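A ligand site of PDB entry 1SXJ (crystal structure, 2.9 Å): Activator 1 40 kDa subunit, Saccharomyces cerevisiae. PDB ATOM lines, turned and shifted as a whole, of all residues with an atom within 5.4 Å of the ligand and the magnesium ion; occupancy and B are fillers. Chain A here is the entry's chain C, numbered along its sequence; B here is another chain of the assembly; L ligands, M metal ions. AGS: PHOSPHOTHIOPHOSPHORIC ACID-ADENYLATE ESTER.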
ATOM      1  N   TRP A  15      -8.029 -25.877  21.152  1.00  0.00           N
ATOM      2  CA  TRP A  15      -8.006 -25.042  19.960  1.00  0.00           C
ATOM      3  C   TRP A  15      -8.268 -23.551  20.196  1.00  0.00           C
ATOM      4  O   TRP A  15      -7.571 -22.695  19.651  1.00  0.00           O
ATOM      5  CB  TRP A  15      -9.033 -25.581  18.961  1.00  0.00           C
ATOM      6  CG  TRP A  15      -8.678 -26.923  18.429  1.00  0.00           C
ATOM      7  CD1 TRP A  15      -7.706 -27.761  18.890  1.00  0.00           C
ATOM      8  CD2 TRP A  15      -9.302 -27.602  17.337  1.00  0.00           C
ATOM      9  NE1 TRP A  15      -7.668 -28.903  18.140  1.00  0.00           N
ATOM     10  CE2 TRP A  15      -8.648 -28.831  17.180  1.00  0.00           C
ATOM     11  CE3 TRP A  15     -10.349 -27.276  16.462  1.00  0.00           C
ATOM     12  CZ2 TRP A  15      -8.998 -29.755  16.185  1.00  0.00           C
ATOM     13  CZ3 TRP A  15     -10.699 -28.190  15.478  1.00  0.00           C
ATOM     14  CH2 TRP A  15     -10.025 -29.410  15.340  1.00  0.00           C
ATOM     15  N   VAL A  16      -9.280 -23.272  21.021  1.00  0.00           N
ATOM     16  CA  VAL A  16      -9.653 -21.901  21.365  1.00  0.00           C
ATOM     17  C   VAL A  16      -8.421 -21.071  21.729  1.00  0.00           C
ATOM     18  O   VAL A  16      -8.340 -19.889  21.395  1.00  0.00           O
ATOM     19  CB  VAL A  16     -10.621 -21.890  22.556  1.00  0.00           C
ATOM     20  CG1 VAL A  16     -11.078 -20.488  22.824  1.00  0.00           C
ATOM     21  CG2 VAL A  16     -11.797 -22.801  22.265  1.00  0.00           C
ATOM     22  N   GLU A  17      -7.479 -21.702  22.413  1.00  0.00           N
ATOM     23  CA  GLU A  17      -6.239 -21.044  22.808  1.00  0.00           C
ATOM     24  C   GLU A  17      -5.140 -21.382  21.827  1.00  0.00           C
ATOM     25  O   GLU A  17      -4.326 -20.530  21.457  1.00  0.00           O
ATOM     26  CB  GLU A  17      -5.828 -21.512  24.212  1.00  0.00           C
ATOM     27  CG  GLU A  17      -6.623 -20.869  25.347  1.00  0.00           C
ATOM     28  CD  GLU A  17      -6.327 -19.382  25.490  1.00  0.00           C
ATOM     29  OE1 GLU A  17      -5.186 -19.036  25.834  1.00  0.00           O
ATOM     30  OE2 GLU A  17      -7.249 -18.574  25.256  1.00  0.00           O
ATOM     31  N   TYR A  19      -4.914 -21.728  18.614  1.00  0.00           N
ATOM     32  CA  TYR A  19      -4.792 -20.851  17.451  1.00  0.00           C
ATOM     33  C   TYR A  19      -4.861 -19.356  17.739  1.00  0.00           C
ATOM     34  O   TYR A  19      -5.441 -18.587  16.979  1.00  0.00           O
ATOM     35  CB  TYR A  19      -5.857 -21.219  16.412  1.00  0.00           C
ATOM     36  CG  TYR A  19      -5.617 -22.560  15.774  1.00  0.00           C
ATOM     37  CD1 TYR A  19      -4.538 -22.765  14.920  1.00  0.00           C
ATOM     38  CD2 TYR A  19      -6.454 -23.638  16.053  1.00  0.00           C
ATOM     39  CE1 TYR A  19      -4.288 -24.019  14.366  1.00  0.00           C
ATOM     40  CE2 TYR A  19      -6.214 -24.894  15.509  1.00  0.00           C
ATOM     41  CZ  TYR A  19      -5.126 -25.079  14.666  1.00  0.00           C
ATOM     42  OH  TYR A  19      -4.896 -26.325  14.123  1.00  0.00           O
ATOM     43  N   ARG A  20      -4.256 -18.949  18.848  1.00  0.00           N
ATOM     44  CA  ARG A  20      -4.237 -17.557  19.258  1.00  0.00           C
ATOM     45  C   ARG A  20      -3.174 -16.757  18.526  1.00  0.00           C
ATOM     46  O   ARG A  20      -1.987 -17.076  18.604  1.00  0.00           O
ATOM     47  CB  ARG A  20      -4.013 -17.487  20.776  1.00  0.00           C
ATOM     48  CG  ARG A  20      -3.365 -16.205  21.266  1.00  0.00           C
ATOM     49  CD  ARG A  20      -3.546 -16.059  22.764  1.00  0.00           C
ATOM     50  NE  ARG A  20      -4.922 -15.677  23.087  1.00  0.00           N
ATOM     51  CZ  ARG A  20      -5.483 -15.830  24.273  1.00  0.00           C
ATOM     52  NH1 ARG A  20      -4.793 -16.386  25.271  1.00  0.00           N
ATOM     53  NH2 ARG A  20      -6.733 -15.437  24.472  1.00  0.00           N
ATOM     54  N   PRO A  21      -3.574 -15.712  17.782  1.00  0.00           N
ATOM     55  CA  PRO A  21      -2.612 -14.905  17.044  1.00  0.00           C
ATOM     56  C   PRO A  21      -1.331 -14.676  17.817  1.00  0.00           C
ATOM     57  O   PRO A  21      -1.368 -14.205  18.954  1.00  0.00           O
ATOM     58  CB  PRO A  21      -3.384 -13.609  16.798  1.00  0.00           C
ATOM     59  CG  PRO A  21      -4.755 -14.109  16.546  1.00  0.00           C
ATOM     60  CD  PRO A  21      -4.943 -15.175  17.632  1.00  0.00           C
ATOM     61  N   GLU A  26      -1.466 -12.112  12.330  1.00  0.00           N
ATOM     62  CA  GLU A  26      -2.284 -13.303  12.482  1.00  0.00           C
ATOM     63  C   GLU A  26      -3.689 -13.013  12.992  1.00  0.00           C
ATOM     64  O   GLU A  26      -4.465 -13.936  13.217  1.00  0.00           O
ATOM     65  CB  GLU A  26      -1.598 -14.298  13.427  1.00  0.00           C
ATOM     66  CG  GLU A  26      -0.284 -14.861  12.887  1.00  0.00           C
ATOM     67  CD  GLU A  26       0.313 -15.928  13.792  1.00  0.00           C
ATOM     68  OE1 GLU A  26      -0.319 -17.002  13.943  1.00  0.00           O
ATOM     69  OE2 GLU A  26       1.396 -15.685  14.363  1.00  0.00           O
ATOM     70  N   VAL A  27      -4.024 -11.732  13.170  1.00  0.00           N
ATOM     71  CA  VAL A  27      -5.354 -11.356  13.642  1.00  0.00           C
ATOM     72  C   VAL A  27      -6.247 -11.177  12.423  1.00  0.00           C
ATOM     73  O   VAL A  27      -5.921 -10.416  11.516  1.00  0.00           O
ATOM     74  CB  VAL A  27      -5.347 -10.036  14.459  1.00  0.00           C
ATOM     75  CG1 VAL A  27      -6.766  -9.584  14.748  1.00  0.00           C
ATOM     76  CG2 VAL A  27      -4.570 -10.224  15.762  1.00  0.00           C
ATOM     77  N   TYR A  28      -7.382 -11.880  12.392  1.00  0.00           N
ATOM     78  CA  TYR A  28      -8.288 -11.796  11.259  1.00  0.00           C
ATOM     79  C   TYR A  28      -9.490 -10.870  11.452  1.00  0.00           C
ATOM     80  O   TYR A  28     -10.114 -10.828  12.511  1.00  0.00           O
ATOM     81  CB  TYR A  28      -8.805 -13.201  10.918  1.00  0.00           C
ATOM     82  CG  TYR A  28      -7.744 -14.167  10.417  1.00  0.00           C
ATOM     83  CD1 TYR A  28      -7.725 -14.599   9.092  1.00  0.00           C
ATOM     84  CD2 TYR A  28      -6.771 -14.665  11.276  1.00  0.00           C
ATOM     85  CE1 TYR A  28      -6.765 -15.490   8.629  1.00  0.00           C
ATOM     86  CE2 TYR A  28      -5.800 -15.557  10.832  1.00  0.00           C
ATOM     87  CZ  TYR A  28      -5.802 -15.970   9.509  1.00  0.00           C
ATOM     88  OH  TYR A  28      -4.832 -16.841   9.067  1.00  0.00           O
ATOM     89  N   GLY A  29      -9.800 -10.106  10.401  1.00  0.00           N
ATOM     90  CA  GLY A  29     -10.945  -9.230  10.439  1.00  0.00           C
ATOM     91  C   GLY A  29     -10.923  -7.982  11.313  1.00  0.00           C
ATOM     92  O   GLY A  29     -11.973  -7.459  11.660  1.00  0.00           O
ATOM     93  N   GLN A  30      -9.738  -7.503  11.661  1.00  0.00           N
ATOM     94  CA  GLN A  30      -9.657  -6.289  12.461  1.00  0.00           C
ATOM     95  C   GLN A  30      -8.594  -5.404  11.833  1.00  0.00           C
ATOM     96  O   GLN A  30      -7.971  -4.584  12.511  1.00  0.00           O
ATOM     97  CB  GLN A  30      -9.270  -6.610  13.912  1.00  0.00           C
ATOM     98  CG  GLN A  30     -10.185  -7.595  14.640  1.00  0.00           C
ATOM     99  CD  GLN A  30     -11.633  -7.113  14.731  1.00  0.00           C
ATOM    100  OE1 GLN A  30     -11.952  -5.984  14.359  1.00  0.00           O
ATOM    101  NE2 GLN A  30     -12.501  -7.974  15.232  1.00  0.00           N
ATOM    102  N   GLY A  53     -15.389  -4.467  22.205  1.00  0.00           N
ATOM    103  CA  GLY A  53     -16.090  -5.328  21.267  1.00  0.00           C
ATOM    104  C   GLY A  53     -16.656  -6.538  21.979  1.00  0.00           C
ATOM    105  O   GLY A  53     -16.446  -6.683  23.186  1.00  0.00           O
ATOM    106  N   PRO A  54     -17.368  -7.421  21.271  1.00  0.00           N
ATOM    107  CA  PRO A  54     -17.948  -8.598  21.906  1.00  0.00           C
ATOM    108  C   PRO A  54     -16.884  -9.654  22.182  1.00  0.00           C
ATOM    109  O   PRO A  54     -15.700  -9.455  21.926  1.00  0.00           O
ATOM    110  CB  PRO A  54     -18.968  -9.086  20.889  1.00  0.00           C
ATOM    111  CG  PRO A  54     -19.169  -7.913  19.974  1.00  0.00           C
ATOM    112  CD  PRO A  54     -17.803  -7.335  19.880  1.00  0.00           C
ATOM    113  N   PRO A  55     -17.309 -10.810  22.712  1.00  0.00           N
ATOM    114  CA  PRO A  55     -16.363 -11.892  23.011  1.00  0.00           C
ATOM    115  C   PRO A  55     -15.654 -12.472  21.782  1.00  0.00           C
ATOM    116  O   PRO A  55     -16.223 -12.538  20.689  1.00  0.00           O
ATOM    117  CB  PRO A  55     -17.237 -12.914  23.726  1.00  0.00           C
ATOM    118  CG  PRO A  55     -18.238 -12.046  24.419  1.00  0.00           C
ATOM    119  CD  PRO A  55     -18.607 -11.083  23.340  1.00  0.00           C
ATOM    120  N   GLY A  56     -14.408 -12.896  21.973  1.00  0.00           N
ATOM    121  CA  GLY A  56     -13.622 -13.502  20.920  1.00  0.00           C
ATOM    122  C   GLY A  56     -13.580 -12.751  19.603  1.00  0.00           C
ATOM    123  O   GLY A  56     -14.038 -13.267  18.583  1.00  0.00           O
ATOM    124  N   THR A  57     -13.027 -11.548  19.612  1.00  0.00           N
ATOM    125  CA  THR A  57     -12.944 -10.731  18.418  1.00  0.00           C
ATOM    126  C   THR A  57     -11.485 -10.401  18.137  1.00  0.00           C
ATOM    127  O   THR A  57     -11.145  -9.862  17.089  1.00  0.00           O
ATOM    128  CB  THR A  57     -13.731  -9.437  18.583  1.00  0.00           C
ATOM    129  OG1 THR A  57     -14.759  -9.637  19.555  1.00  0.00           O
ATOM    130  CG2 THR A  57     -14.385  -9.045  17.296  1.00  0.00           C
ATOM    131  N   GLY A  58     -10.626 -10.719  19.109  1.00  0.00           N
ATOM    132  CA  GLY A  58      -9.200 -10.475  18.936  1.00  0.00           C
ATOM    133  C   GLY A  58      -8.612  -9.374  19.780  1.00  0.00           C
ATOM    134  O   GLY A  58      -7.440  -9.020  19.612  1.00  0.00           O
ATOM    135  N   LYS A  59      -9.400  -8.831  20.710  1.00  0.00           N
ATOM    136  CA  LYS A  59      -8.921  -7.755  21.577  1.00  0.00           C
ATOM    137  C   LYS A  59      -7.666  -8.080  22.393  1.00  0.00           C
ATOM    138  O   LYS A  59      -6.657  -7.384  22.269  1.00  0.00           O
ATOM    139  CB  LYS A  59     -10.046  -7.296  22.516  1.00  0.00           C
ATOM    140  CG  LYS A  59     -11.068  -6.399  21.859  1.00  0.00           C
ATOM    141  CD  LYS A  59     -12.045  -5.818  22.878  1.00  0.00           C
ATOM    142  CE  LYS A  59     -13.388  -6.550  22.874  1.00  0.00           C
ATOM    143  NZ  LYS A  59     -13.296  -7.951  23.291  1.00  0.00           N
ATOM    144  N   THR A  60      -7.724  -9.117  23.215  1.00  0.00           N
ATOM    145  CA  THR A  60      -6.558  -9.475  24.024  1.00  0.00           C
ATOM    146  C   THR A  60      -5.392  -9.914  23.115  1.00  0.00           C
ATOM    147  O   THR A  60      -4.226  -9.561  23.347  1.00  0.00           O
ATOM    148  CB  THR A  60      -6.907 -10.583  25.044  1.00  0.00           C
ATOM    149  OG1 THR A  60      -7.853 -10.087  25.987  1.00  0.00           O
ATOM    150  CG2 THR A  60      -5.649 -11.044  25.783  1.00  0.00           C
ATOM    151  N   SER A  61      -5.721 -10.664  22.068  1.00  0.00           N
ATOM    152  CA  SER A  61      -4.705 -11.139  21.142  1.00  0.00           C
ATOM    153  C   SER A  61      -3.952  -9.940  20.602  1.00  0.00           C
ATOM    154  O   SER A  61      -2.731  -9.913  20.606  1.00  0.00           O
ATOM    155  CB  SER A  61      -5.359 -11.885  19.968  1.00  0.00           C
ATOM    156  OG  SER A  61      -6.069 -13.036  20.389  1.00  0.00           O
ATOM    157  N   THR A  62      -4.699  -8.934  20.171  1.00  0.00           N
ATOM    158  CA  THR A  62      -4.138  -7.730  19.588  1.00  0.00           C
ATOM    159  C   THR A  62      -3.159  -6.895  20.434  1.00  0.00           C
ATOM    160  O   THR A  62      -2.090  -6.547  19.929  1.00  0.00           O
ATOM    161  CB  THR A  62      -5.256  -6.803  19.057  1.00  0.00           C
ATOM    162  OG1 THR A  62      -6.073  -7.537  18.120  1.00  0.00           O
ATOM    163  CG2 THR A  62      -4.660  -5.582  18.354  1.00  0.00           C
ATOM    164  N   ASP A 117      -6.917  -5.100  31.001  1.00  0.00           N
ATOM    165  CA  ASP A 117      -7.869  -5.962  30.304  1.00  0.00           C
ATOM    166  C   ASP A 117      -9.159  -6.042  31.091  1.00  0.00           C
ATOM    167  O   ASP A 117      -9.159  -5.916  32.320  1.00  0.00           O
ATOM    168  CB  ASP A 117      -7.280  -7.353  30.111  1.00  0.00           C
ATOM    169  CG  ASP A 117      -7.558  -7.923  28.730  1.00  0.00           C
ATOM    170  OD1 ASP A 117      -8.726  -7.926  28.304  1.00  0.00           O
ATOM    171  OD2 ASP A 117      -6.593  -8.364  28.079  1.00  0.00           O
ATOM    172  N   GLU A 118     -10.257  -6.278  30.381  1.00  0.00           N
ATOM    173  CA  GLU A 118     -11.585  -6.330  30.981  1.00  0.00           C
ATOM    174  C   GLU A 118     -11.721  -5.227  32.024  1.00  0.00           C
ATOM    175  O   GLU A 118     -12.110  -5.451  33.170  1.00  0.00           O
ATOM    176  CB  GLU A 118     -11.858  -7.724  31.573  1.00  0.00           C
ATOM    177  CG  GLU A 118     -10.611  -8.450  32.009  1.00  0.00           C
ATOM    178  CD  GLU A 118     -10.590  -9.898  31.544  1.00  0.00           C
ATOM    179  OE1 GLU A 118      -9.627 -10.621  31.891  1.00  0.00           O
ATOM    180  OE2 GLU A 118     -11.531 -10.308  30.829  1.00  0.00           O
ATOM    181  N   ASN A 148     -15.804  -5.085  26.849  1.00  0.00           N
ATOM    182  CA  ASN A 148     -16.865  -5.603  26.013  1.00  0.00           C
ATOM    183  C   ASN A 148     -17.917  -4.521  25.817  1.00  0.00           C
ATOM    184  O   ASN A 148     -18.608  -4.475  24.805  1.00  0.00           O
ATOM    185  CB  ASN A 148     -17.484  -6.832  26.646  1.00  0.00           C
ATOM    186  CG  ASN A 148     -16.556  -8.008  26.631  1.00  0.00           C
ATOM    187  OD1 ASN A 148     -16.069  -8.444  27.672  1.00  0.00           O
ATOM    188  ND2 ASN A 148     -16.288  -8.547  25.441  1.00  0.00           N
ATOM    189  N   LEU A 169     -16.251 -10.948  13.776  1.00  0.00           N
ATOM    190  CA  LEU A 169     -15.504 -11.430  12.610  1.00  0.00           C
ATOM    191  C   LEU A 169     -16.419 -11.674  11.421  1.00  0.00           C
ATOM    192  O   LEU A 169     -17.377 -12.427  11.511  1.00  0.00           O
ATOM    193  CB  LEU A 169     -14.749 -12.702  12.948  1.00  0.00           C
ATOM    194  CG  LEU A 169     -13.568 -12.546  13.912  1.00  0.00           C
ATOM    195  CD1 LEU A 169     -12.772 -11.312  13.502  1.00  0.00           C
ATOM    196  CD2 LEU A 169     -14.083 -12.389  15.332  1.00  0.00           C
ATOM    197  N   ARG A 177      -9.742 -18.372   8.680  1.00  0.00           N
ATOM    198  CA  ARG A 177      -9.210 -19.131   9.793  1.00  0.00           C
ATOM    199  C   ARG A 177      -9.644 -20.597   9.737  1.00  0.00           C
ATOM    200  O   ARG A 177      -8.864 -21.497  10.072  1.00  0.00           O
ATOM    201  CB  ARG A 177      -9.646 -18.515  11.124  1.00  0.00           C
ATOM    202  CG  ARG A 177      -8.861 -19.027  12.300  1.00  0.00           C
ATOM    203  CD  ARG A 177      -7.375 -18.857  12.050  1.00  0.00           C
ATOM    204  NE  ARG A 177      -6.608 -18.842  13.294  1.00  0.00           N
ATOM    205  CZ  ARG A 177      -5.288 -18.754  13.347  1.00  0.00           C
ATOM    206  NH1 ARG A 177      -4.582 -18.679  12.221  1.00  0.00           N
ATOM    207  NH2 ARG A 177      -4.675 -18.721  14.517  1.00  0.00           N
ATOM    208  N   MET A 205     -15.133 -15.717  16.909  1.00  0.00           N
ATOM    209  CA  MET A 205     -14.117 -16.690  16.510  1.00  0.00           C
ATOM    210  C   MET A 205     -13.945 -17.779  17.551  1.00  0.00           C
ATOM    211  O   MET A 205     -13.601 -18.922  17.230  1.00  0.00           O
ATOM    212  CB  MET A 205     -12.781 -15.977  16.304  1.00  0.00           C
ATOM    213  CG  MET A 205     -11.651 -16.872  15.854  1.00  0.00           C
ATOM    214  SD  MET A 205     -11.784 -17.379  14.130  1.00  0.00           S
ATOM    215  CE  MET A 205     -12.188 -19.109  14.329  1.00  0.00           C
ATOM    216  N   ARG A 206     -14.193 -17.433  18.810  1.00  0.00           N
ATOM    217  CA  ARG A 206     -14.044 -18.395  19.889  1.00  0.00           C
ATOM    218  C   ARG A 206     -14.993 -19.587  19.745  1.00  0.00           C
ATOM    219  O   ARG A 206     -14.581 -20.731  19.902  1.00  0.00           O
ATOM    220  CB  ARG A 206     -14.243 -17.691  21.244  1.00  0.00           C
ATOM    221  CG  ARG A 206     -13.406 -18.270  22.385  1.00  0.00           C
ATOM    222  CD  ARG A 206     -13.894 -17.818  23.760  1.00  0.00           C
ATOM    223  NE  ARG A 206     -13.556 -16.442  24.126  1.00  0.00           N
ATOM    224  CZ  ARG A 206     -12.363 -16.058  24.570  1.00  0.00           C
ATOM    225  NH1 ARG A 206     -11.381 -16.940  24.718  1.00  0.00           N
ATOM    226  NH2 ARG A 206     -12.162 -14.784  24.887  1.00  0.00           N
ATOM    227  N   LEU A 209     -13.817 -22.212  16.752  1.00  0.00           N
ATOM    228  CA  LEU A 209     -12.736 -23.112  17.115  1.00  0.00           C
ATOM    229  C   LEU A 209     -13.187 -24.134  18.144  1.00  0.00           C
ATOM    230  O   LEU A 209     -12.609 -25.220  18.247  1.00  0.00           O
ATOM    231  CB  LEU A 209     -11.555 -22.324  17.670  1.00  0.00           C
ATOM    232  CG  LEU A 209     -10.878 -21.394  16.669  1.00  0.00           C
ATOM    233  CD1 LEU A 209      -9.823 -20.560  17.391  1.00  0.00           C
ATOM    234  CD2 LEU A 209     -10.256 -22.204  15.541  1.00  0.00           C
ATOM    235  N   ARG B 154     -12.324 -15.347  34.274  1.00  0.00           N
ATOM    236  CA  ARG B 154     -11.868 -15.257  32.878  1.00  0.00           C
ATOM    237  C   ARG B 154     -10.400 -15.482  32.509  1.00  0.00           C
ATOM    238  O   ARG B 154     -10.067 -16.534  31.972  1.00  0.00           O
ATOM    239  CB  ARG B 154     -12.353 -13.942  32.281  1.00  0.00           C
ATOM    240  CG  ARG B 154     -13.492 -14.146  31.323  1.00  0.00           C
ATOM    241  CD  ARG B 154     -13.663 -12.935  30.449  1.00  0.00           C
ATOM    242  NE  ARG B 154     -14.241 -11.823  31.189  1.00  0.00           N
ATOM    243  CZ  ARG B 154     -14.429 -10.612  30.686  1.00  0.00           C
ATOM    244  NH1 ARG B 154     -14.075 -10.344  29.443  1.00  0.00           N
ATOM    245  NH2 ARG B 154     -14.990  -9.670  31.437  1.00  0.00           N
ATOM    246  N   GLU B 158      -8.002 -19.225  31.275  1.00  0.00           N
ATOM    247  CA  GLU B 158      -7.662 -18.999  29.880  1.00  0.00           C
ATOM    248  C   GLU B 158      -6.162 -19.122  29.686  1.00  0.00           C
ATOM    249  O   GLU B 158      -5.697 -19.654  28.679  1.00  0.00           O
ATOM    250  CB  GLU B 158      -8.154 -17.622  29.438  1.00  0.00           C
ATOM    251  CG  GLU B 158      -7.871 -17.296  27.980  1.00  0.00           C
ATOM    252  CD  GLU B 158      -8.481 -15.982  27.519  1.00  0.00           C
ATOM    253  OE1 GLU B 158      -8.228 -14.945  28.182  1.00  0.00           O
ATOM    254  OE2 GLU B 158      -9.200 -15.977  26.495  1.00  0.00           O
ATOM    255  N   PRO B 179     -18.722 -13.387  28.289  1.00  0.00           N
ATOM    256  CA  PRO B 179     -17.321 -13.766  28.125  1.00  0.00           C
ATOM    257  C   PRO B 179     -17.040 -15.244  28.420  1.00  0.00           C
ATOM    258  O   PRO B 179     -16.422 -15.930  27.610  1.00  0.00           O
ATOM    259  CB  PRO B 179     -16.603 -12.826  29.076  1.00  0.00           C
ATOM    260  CG  PRO B 179     -17.380 -11.575  28.909  1.00  0.00           C
ATOM    261  CD  PRO B 179     -18.819 -12.084  28.969  1.00  0.00           C
ATOM    262  N   SER B 182     -18.478 -17.843  26.262  1.00  0.00           N
ATOM    263  CA  SER B 182     -17.671 -17.869  25.046  1.00  0.00           C
ATOM    264  C   SER B 182     -16.534 -18.856  25.203  1.00  0.00           C
ATOM    265  O   SER B 182     -16.301 -19.694  24.340  1.00  0.00           O
ATOM    266  CB  SER B 182     -17.127 -16.451  24.766  1.00  0.00           C
ATOM    267  OG  SER B 182     -16.569 -16.322  23.468  1.00  0.00           O
HETATM  268  PG  AGS L   1     -13.021 -11.494  25.547  1.00  0.00           P
HETATM  269  S1G AGS L   1     -13.680  -9.938  25.380  1.00  0.00           S
HETATM  270  O2G AGS L   1     -14.062 -12.557  25.754  1.00  0.00           O
HETATM  271  O3G AGS L   1     -12.035 -11.489  26.751  1.00  0.00           O
HETATM  272  PB  AGS L   1     -11.106 -11.123  23.276  1.00  0.00           P
HETATM  273  O1B AGS L   1     -10.088 -10.644  24.263  1.00  0.00           O
HETATM  274  O2B AGS L   1     -11.652 -10.151  22.294  1.00  0.00           O
HETATM  275  O3B AGS L   1     -12.260 -11.802  24.119  1.00  0.00           O
HETATM  276  PA  AGS L   1      -9.067 -13.085  22.407  1.00  0.00           P
HETATM  277  O1A AGS L   1      -8.579 -13.527  23.758  1.00  0.00           O
HETATM  278  O2A AGS L   1      -8.160 -12.112  21.709  1.00  0.00           O
HETATM  279  O3A AGS L   1     -10.514 -12.373  22.499  1.00  0.00           O
HETATM  280  O5' AGS L   1      -9.464 -14.302  21.439  1.00  0.00           O
HETATM  281  C5' AGS L   1      -9.740 -15.588  22.067  1.00  0.00           C
HETATM  282  C4' AGS L   1      -9.338 -16.727  21.142  1.00  0.00           C
HETATM  283  O4' AGS L   1     -10.150 -16.585  19.918  1.00  0.00           O
HETATM  284  C3' AGS L   1      -7.866 -16.666  20.667  1.00  0.00           C
HETATM  285  O3' AGS L   1      -6.983 -17.512  21.402  1.00  0.00           O
HETATM  286  C2' AGS L   1      -7.930 -16.951  19.152  1.00  0.00           C
HETATM  287  O2' AGS L   1      -7.532 -18.258  18.750  1.00  0.00           O
HETATM  288  C1' AGS L   1      -9.349 -16.673  18.730  1.00  0.00           C
HETATM  289  N9  AGS L   1      -9.500 -15.356  17.961  1.00  0.00           N
HETATM  290  C8  AGS L   1     -10.336 -14.338  18.395  1.00  0.00           C
HETATM  291  N7  AGS L   1     -10.378 -13.258  17.629  1.00  0.00           N
HETATM  292  C5  AGS L   1      -9.513 -13.553  16.609  1.00  0.00           C
HETATM  293  C6  AGS L   1      -9.074 -12.834  15.426  1.00  0.00           C
HETATM  294  N6  AGS L   1      -9.497 -11.591  15.104  1.00  0.00           N
HETATM  295  N1  AGS L   1      -8.169 -13.458  14.597  1.00  0.00           N
HETATM  296  C2  AGS L   1      -7.726 -14.719  14.898  1.00  0.00           C
HETATM  297  N3  AGS L   1      -8.056 -15.498  15.963  1.00  0.00           N
HETATM  298  C4  AGS L   1      -8.962 -14.864  16.792  1.00  0.00           C
HETATM  299 MG    MG M   1     -10.035 -10.724  26.421  1.00  0.00          MG
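The backbone carbonyl oxygen of Tyr 19 is in hydrogen-bond range of an oxygen (O2') of the ligand, at 2.8 Å. The backbone carbonyl oxygen (O) of Val 16 is in hydrogen-bond range of an oxygen (O3') of the ligand, 2.7 Å away. A nitrogen (N6) of the ligand sits at hydrogen-bond distance from the backbone carbonyl oxygen (O) of Thr 57, 3.1 Å away. The side-chain amino group (NZ) of Lys 59 lies within salt-bridge range of an oxygen (O2B) of the ligand. O2B of the ligand sits at hydrogen-bond distance from N of Lys 59, at 3.1 Å. O2B of the ligand sits at hydrogen-bond distance from N of Thr 57, at 3.3 Å. O2A of the ligand sits at hydrogen-bond distance from N of Ser 61. An oxygen (O2') of the ligand lies within hydrogen-bond range of the backbone NH of Arg 20 (3.3 Å). ND2 of Asn 148 sits close to S1G of the ligand, at 3.0 Å. The guanidinium group (NH2) of Arg 206 is in salt-bridge range of an oxygen (O1A) of the ligand. The guanidinium group of Arg 20 lies within salt-bridge range of an oxygen (O1A) of the ligand, 2.8 Å away. An oxygen (O3B) of the ligand is in hydrogen-bond range of the backbone NH (N) of Gly 56 (3.2 Å). A nitrogen (N1) of the ligand lies within hydrogen-bond range of the backbone NH (N) of Tyr 28. The backbone carbonyl oxygen (O) of Tyr 28 sits at hydrogen-bond distance from a nitrogen (N6) of the ligand (2.8 Å). The backbone NH (N) of Gly 58 is in hydrogen-bond range of a nitrogen (N7) of the ligand (2.9 Å). The side-chain hydroxyl of Ser 61 lies within hydrogen-bond range of an oxygen (O2A) of the ligand (2.6 Å). The backbone NH (N) of Thr 60 sits at hydrogen-bond distance from an oxygen (O2A) of the ligand.
The side-chain amide nitrogen (ND2) of Asn 148 sits at hydrogen-bond distance from the backbone carbonyl oxygen (O) of Gly 53. The guanidinium group (NH1) of Arg 206 is in salt-bridge range of the side-chain carboxylate (OE2) of Glu 158 of chain B (3.0 Å). The side-chain hydroxyl (OG1) of Thr 60 sits close to the side-chain carboxylate (OD2) of Asp 117. The side-chain amide oxygen (OD1) of Asn 148 is in hydrogen-bond range of the guanidinium group (NH1) of Arg 154 of chain B. The backbone carbonyl oxygen of Gly 58 sits at hydrogen-bond distance from the side-chain hydroxyl of Thr 62. The side-chain carboxylate (OE1) of Glu 17 is in salt-bridge range of the guanidinium group (NH1) of Arg 20, 2.7 Å away. NE2 of Gln 30 is in hydrogen-bond range of O of Thr 57 (3.0 Å). O of Tyr 19 lies within hydrogen-bond range of NH2 of Arg 177.
CA of Glu 17 touches O3' of the ligand, at 3.9 Å. CG of Pro 21 touches C2 of the ligand, 3.5 Å away. Glu 26 touches the ligand (O to C2, 3.8 Å). Val 27 touches the ligand. Pro 55 touches the ligand. Leu 169 touches the ligand (CD1 to N6, 3.7 Å). CG of Met 205 touches N9 of the ligand, 3.4 Å away. Leu 209 touches the ligand (CD1 to O2', 3.5 Å). Arg 154 of chain B touches the ligand (NH1 to O3G, 3.6 Å). Glu 158 of chain B touches the ligand. Hydrophobic or aromatic side chains that line the ligand: Pro 21, Val 27, Tyr 28, Pro 55, Leu 169, Met 205 and Leu 209. Within 4 Å of the ligand: Val 16, Glu 17, Tyr 19, Arg 20, Pro 21, Glu 26, Val 27, Tyr 28, Pro 55, Gly 56, Thr 57, Gly 58, Lys 59, Thr 60, Ser 61, Asn 148, Leu 169, Met 205, Arg 206, Leu 209, Arg 154 of chain B and Glu 158 of chain B. The nearest printed residue that does not touch the ligand is Pro 54 (4.03 Å).
Asp 117 touches the magnesium ion. Within 4 Å of the magnesium ion: Thr 60 and Asp 117. The nearest printed residue that does not touch the magnesium ion is Glu 118 (4.7 Å).
The magnesium ion is bound by an oxygen (O1B) of the ligand (2.2 Å). The magnesium ion is bound by O3G of the ligand. The magnesium ion is bound by OG1 of Thr 60 (2.3 Å).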
